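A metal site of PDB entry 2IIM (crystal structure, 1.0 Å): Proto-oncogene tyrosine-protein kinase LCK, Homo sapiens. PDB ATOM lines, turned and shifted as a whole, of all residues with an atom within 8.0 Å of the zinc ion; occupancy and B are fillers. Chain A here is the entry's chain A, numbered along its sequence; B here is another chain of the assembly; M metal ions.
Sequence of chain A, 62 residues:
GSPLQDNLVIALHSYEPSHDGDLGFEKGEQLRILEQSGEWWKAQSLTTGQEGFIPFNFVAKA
Within 4 Å of the zinc ion: His 19, Asp 22 and His 13 of chain B. The nearest printed residue that does not touch the zinc ion is Trp 40 (4.2 Å).
The zinc ion is bound by ND1 of His 19 (2.0 Å). A ring nitrogen (NE2) of His 13 of chain B binds the zinc ion (2.0 Å). OD2 of Asp 22 binds the zinc ion (2.1 Å).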
ATOM      1  N   TYR A  15     -20.658  22.269   2.451  1.00  0.00           N
ATOM      2  CA  TYR A  15     -20.440  22.976   1.189  1.00  0.00           C
ATOM      3  C   TYR A  15     -20.307  21.937   0.086  1.00  0.00           C
ATOM      4  O   TYR A  15     -19.535  20.980   0.216  1.00  0.00           O
ATOM      5  CB  TYR A  15     -19.193  23.898   1.257  1.00  0.00           C
ATOM      6  CG  TYR A  15     -19.048  24.647  -0.050  1.00  0.00           C
ATOM      7  CD1 TYR A  15     -20.075  25.487  -0.471  1.00  0.00           C
ATOM      8  CD2 TYR A  15     -17.942  24.472  -0.884  1.00  0.00           C
ATOM      9  CE1 TYR A  15     -19.997  26.179  -1.669  1.00  0.00           C
ATOM     10  CE2 TYR A  15     -17.904  25.139  -2.119  1.00  0.00           C
ATOM     11  CZ  TYR A  15     -18.940  25.982  -2.504  1.00  0.00           C
ATOM     12  OH  TYR A  15     -18.917  26.598  -3.728  1.00  0.00           O
ATOM     13  N   PRO A  17     -19.304  21.858  -3.921  1.00  0.00           N
ATOM     14  CA  PRO A  17     -18.689  22.703  -4.926  1.00  0.00           C
ATOM     15  C   PRO A  17     -19.426  22.620  -6.280  1.00  0.00           C
ATOM     16  O   PRO A  17     -20.133  21.666  -6.564  1.00  0.00           O
ATOM     17  CB  PRO A  17     -17.285  22.178  -5.036  1.00  0.00           C
ATOM     18  CG  PRO A  17     -17.421  20.721  -4.742  1.00  0.00           C
ATOM     19  CD  PRO A  17     -18.489  20.663  -3.682  1.00  0.00           C
ATOM     20  N   SER A  18     -19.208  23.684  -7.056  1.00  0.00           N
ATOM     21  CA  SER A  18     -19.825  23.809  -8.359  1.00  0.00           C
ATOM     22  C   SER A  18     -18.863  24.391  -9.364  1.00  0.00           C
ATOM     23  O   SER A  18     -19.291  25.081 -10.287  1.00  0.00           O
ATOM     24  CB  SER A  18     -21.175  24.542  -8.266  1.00  0.00           C
ATOM     25  OG  SER A  18     -21.036  25.751  -7.549  1.00  0.00           O
ATOM     26  N   HIS A  19     -17.564  24.165  -9.144  1.00  0.00           N
ATOM     27  CA  HIS A  19     -16.493  24.808  -9.914  1.00  0.00           C
ATOM     28  C   HIS A  19     -15.282  23.903  -9.695  1.00  0.00           C
ATOM     29  O   HIS A  19     -14.899  23.614  -8.540  1.00  0.00           O
ATOM     30  CB  HIS A  19     -16.242  26.228  -9.464  1.00  0.00           C
ATOM     31  CG  HIS A  19     -15.055  26.917 -10.002  1.00  0.00           C
ATOM     32  ND1 HIS A  19     -14.462  27.898  -9.259  1.00  0.00           N
ATOM     33  CD2 HIS A  19     -14.390  26.770 -11.160  1.00  0.00           C
ATOM     34  CE1 HIS A  19     -13.407  28.352 -10.006  1.00  0.00           C
ATOM     35  NE2 HIS A  19     -13.345  27.688 -11.152  1.00  0.00           N
ATOM     36  N   ASP A  20     -14.657  23.388 -10.756  1.00  0.00           N
ATOM     37  CA  ASP A  20     -13.511  22.553 -10.648  1.00  0.00           C
ATOM     38  C   ASP A  20     -12.440  23.177  -9.784  1.00  0.00           C
ATOM     39  O   ASP A  20     -12.115  24.359  -9.979  1.00  0.00           O
ATOM     40  CB  ASP A  20     -12.935  22.347 -12.047  1.00  0.00           C
ATOM     41  CG  ASP A  20     -13.750  21.439 -12.928  1.00  0.00           C
ATOM     42  OD1 ASP A  20     -14.799  20.905 -12.561  1.00  0.00           O
ATOM     43  OD2 ASP A  20     -13.236  21.274 -14.031  1.00  0.00           O
ATOM     44  N   GLY A  21     -11.846  22.445  -8.849  1.00  0.00           N
ATOM     45  CA  GLY A  21     -10.804  22.979  -7.984  1.00  0.00           C
ATOM     46  C   GLY A  21     -11.326  23.531  -6.672  1.00  0.00           C
ATOM     47  O   GLY A  21     -10.514  23.832  -5.796  1.00  0.00           O
ATOM     48  N   ASP A  22     -12.632  23.667  -6.529  1.00  0.00           N
ATOM     49  CA  ASP A  22     -13.215  24.061  -5.240  1.00  0.00           C
ATOM     50  C   ASP A  22     -13.467  22.788  -4.439  1.00  0.00           C
ATOM     51  O   ASP A  22     -13.809  21.719  -4.959  1.00  0.00           O
ATOM     52  CB  ASP A  22     -14.464  24.876  -5.444  1.00  0.00           C
ATOM     53  CG  ASP A  22     -14.188  26.241  -6.057  1.00  0.00           C
ATOM     54  OD1 ASP A  22     -13.022  26.658  -6.155  1.00  0.00           O
ATOM     55  OD2 ASP A  22     -15.205  26.940  -6.407  1.00  0.00           O
ATOM     56  N   LEU A  23     -13.330  22.870  -3.132  1.00  0.00           N
ATOM     57  CA  LEU A  23     -13.376  21.742  -2.224  1.00  0.00           C
ATOM     58  C   LEU A  23     -14.670  21.756  -1.419  1.00  0.00           C
ATOM     59  O   LEU A  23     -14.989  22.748  -0.769  1.00  0.00           O
ATOM     60  CB  LEU A  23     -12.188  21.798  -1.272  1.00  0.00           C
ATOM     61  CG  LEU A  23     -12.046  20.752  -0.193  1.00  0.00           C
ATOM     62  CD1 LEU A  23     -11.841  19.358  -0.792  1.00  0.00           C
ATOM     63  CD2 LEU A  23     -10.927  21.050   0.760  1.00  0.00           C
ATOM     64  N   TRP A  40     -11.751  33.171  -0.899  1.00  0.00           N
ATOM     65  CA  TRP A  40     -11.623  31.742  -1.212  1.00  0.00           C
ATOM     66  C   TRP A  40     -10.262  31.289  -0.727  1.00  0.00           C
ATOM     67  O   TRP A  40      -9.229  31.780  -1.185  1.00  0.00           O
ATOM     68  CB  TRP A  40     -11.793  31.475  -2.721  1.00  0.00           C
ATOM     69  CG  TRP A  40     -13.213  31.599  -3.150  1.00  0.00           C
ATOM     70  CD1 TRP A  40     -13.872  32.742  -3.547  1.00  0.00           C
ATOM     71  CD2 TRP A  40     -14.188  30.544  -3.222  1.00  0.00           C
ATOM     72  NE1 TRP A  40     -15.161  32.441  -3.869  1.00  0.00           N
ATOM     73  CE2 TRP A  40     -15.368  31.100  -3.676  1.00  0.00           C
ATOM     74  CE3 TRP A  40     -14.104  29.153  -2.955  1.00  0.00           C
ATOM     75  CZ2 TRP A  40     -16.524  30.343  -3.863  1.00  0.00           C
ATOM     76  CZ3 TRP A  40     -15.244  28.418  -3.158  1.00  0.00           C
ATOM     77  CH2 TRP A  40     -16.446  28.971  -3.607  1.00  0.00           C
ATOM     78  N   PHE A  53     -10.139  25.003  -3.070  1.00  0.00           N
ATOM     79  CA  PHE A  53     -10.555  26.300  -2.545  1.00  0.00           C
ATOM     80  C   PHE A  53     -11.929  26.238  -1.890  1.00  0.00           C
ATOM     81  O   PHE A  53     -12.861  25.590  -2.392  1.00  0.00           O
ATOM     82  CB  PHE A  53     -10.535  27.331  -3.685  1.00  0.00           C
ATOM     83  CG  PHE A  53      -9.139  27.642  -4.102  1.00  0.00           C
ATOM     84  CD1 PHE A  53      -8.385  28.610  -3.457  1.00  0.00           C
ATOM     85  CD2 PHE A  53      -8.544  26.927  -5.143  1.00  0.00           C
ATOM     86  CE1 PHE A  53      -7.089  28.893  -3.812  1.00  0.00           C
ATOM     87  CE2 PHE A  53      -7.229  27.207  -5.512  1.00  0.00           C
ATOM     88  CZ  PHE A  53      -6.517  28.173  -4.833  1.00  0.00           C
ATOM     89  N   ILE A  54     -12.027  26.921  -0.749  1.00  0.00           N
ATOM     90  CA  ILE A  54     -13.224  26.907   0.076  1.00  0.00           C
ATOM     91  C   ILE A  54     -13.719  28.311   0.317  1.00  0.00           C
ATOM     92  O   ILE A  54     -12.924  29.258   0.444  1.00  0.00           O
ATOM     93  CB  ILE A  54     -13.006  26.180   1.409  1.00  0.00           C
ATOM     94  CG1 ILE A  54     -12.032  26.888   2.339  1.00  0.00           C
ATOM     95  CG2 ILE A  54     -12.589  24.728   1.154  1.00  0.00           C
ATOM     96  CD1 ILE A  54     -11.937  26.262   3.734  1.00  0.00           C
ATOM     97  N   PRO A  55     -15.048  28.474   0.473  1.00  0.00           N
ATOM     98  CA  PRO A  55     -15.601  29.784   0.770  1.00  0.00           C
ATOM     99  C   PRO A  55     -15.417  30.100   2.247  1.00  0.00           C
ATOM    100  O   PRO A  55     -15.880  29.352   3.113  1.00  0.00           O
ATOM    101  CB  PRO A  55     -17.078  29.629   0.378  1.00  0.00           C
ATOM    102  CG  PRO A  55     -17.355  28.164   0.577  1.00  0.00           C
ATOM    103  CD  PRO A  55     -16.093  27.474   0.229  1.00  0.00           C
ATOM    104  N   LEU B  12     -22.064  36.156  -8.105  1.00  0.00           N
ATOM    105  CA  LEU B  12     -20.682  36.245  -8.434  1.00  0.00           C
ATOM    106  C   LEU B  12     -20.035  34.893  -8.715  1.00  0.00           C
ATOM    107  O   LEU B  12     -18.974  34.824  -9.354  1.00  0.00           O
ATOM    108  CB  LEU B  12     -19.908  36.859  -7.251  1.00  0.00           C
ATOM    109  CG  LEU B  12     -20.331  38.282  -6.894  1.00  0.00           C
ATOM    110  CD1 LEU B  12     -19.693  38.653  -5.560  1.00  0.00           C
ATOM    111  CD2 LEU B  12     -19.959  39.296  -7.958  1.00  0.00           C
ATOM    112  N   HIS B  13     -20.646  33.836  -8.178  1.00  0.00           N
ATOM    113  CA  HIS B  13     -20.144  32.475  -8.257  1.00  0.00           C
ATOM    114  C   HIS B  13     -21.401  31.576  -8.183  1.00  0.00           C
ATOM    115  O   HIS B  13     -22.384  31.957  -7.522  1.00  0.00           O
ATOM    116  CB  HIS B  13     -19.212  32.199  -7.098  1.00  0.00           C
ATOM    117  CG  HIS B  13     -18.401  30.950  -7.169  1.00  0.00           C
ATOM    118  ND1 HIS B  13     -18.899  29.685  -6.970  1.00  0.00           N
ATOM    119  CD2 HIS B  13     -17.056  30.810  -7.377  1.00  0.00           C
ATOM    120  CE1 HIS B  13     -17.901  28.835  -7.082  1.00  0.00           C
ATOM    121  NE2 HIS B  13     -16.756  29.463  -7.338  1.00  0.00           N
ATOM    122  N   SER B  14     -21.369  30.438  -8.826  1.00  0.00           N
ATOM    123  CA  SER B  14     -22.436  29.468  -8.679  1.00  0.00           C
ATOM    124  C   SER B  14     -22.491  28.930  -7.257  1.00  0.00           C
ATOM    125  O   SER B  14     -21.490  28.942  -6.510  1.00  0.00           O
ATOM    126  CB  SER B  14     -22.257  28.327  -9.672  1.00  0.00           C
ATOM    127  OG  SER B  14     -21.044  27.666  -9.458  1.00  0.00           O
ATOM    128  N   PHE B  58     -21.727  35.198  -1.982  1.00  0.00           N
ATOM    129  CA  PHE B  58     -21.772  34.678  -3.332  1.00  0.00           C
ATOM    130  C   PHE B  58     -22.491  35.615  -4.291  1.00  0.00           C
ATOM    131  O   PHE B  58     -22.521  35.332  -5.501  1.00  0.00           O
ATOM    132  CB  PHE B  58     -22.433  33.317  -3.372  1.00  0.00           C
ATOM    133  CG  PHE B  58     -21.550  32.153  -2.964  1.00  0.00           C
ATOM    134  CD1 PHE B  58     -21.004  32.071  -1.684  1.00  0.00           C
ATOM    135  CD2 PHE B  58     -21.257  31.134  -3.853  1.00  0.00           C
ATOM    136  CE1 PHE B  58     -20.177  31.002  -1.344  1.00  0.00           C
ATOM    137  CE2 PHE B  58     -20.469  30.076  -3.512  1.00  0.00           C
ATOM    138  CZ  PHE B  58     -19.930  30.006  -2.237  1.00  0.00           C
HETATM  139 ZN    ZN M   1     -14.913  28.666  -7.475  1.00  0.00          ZN
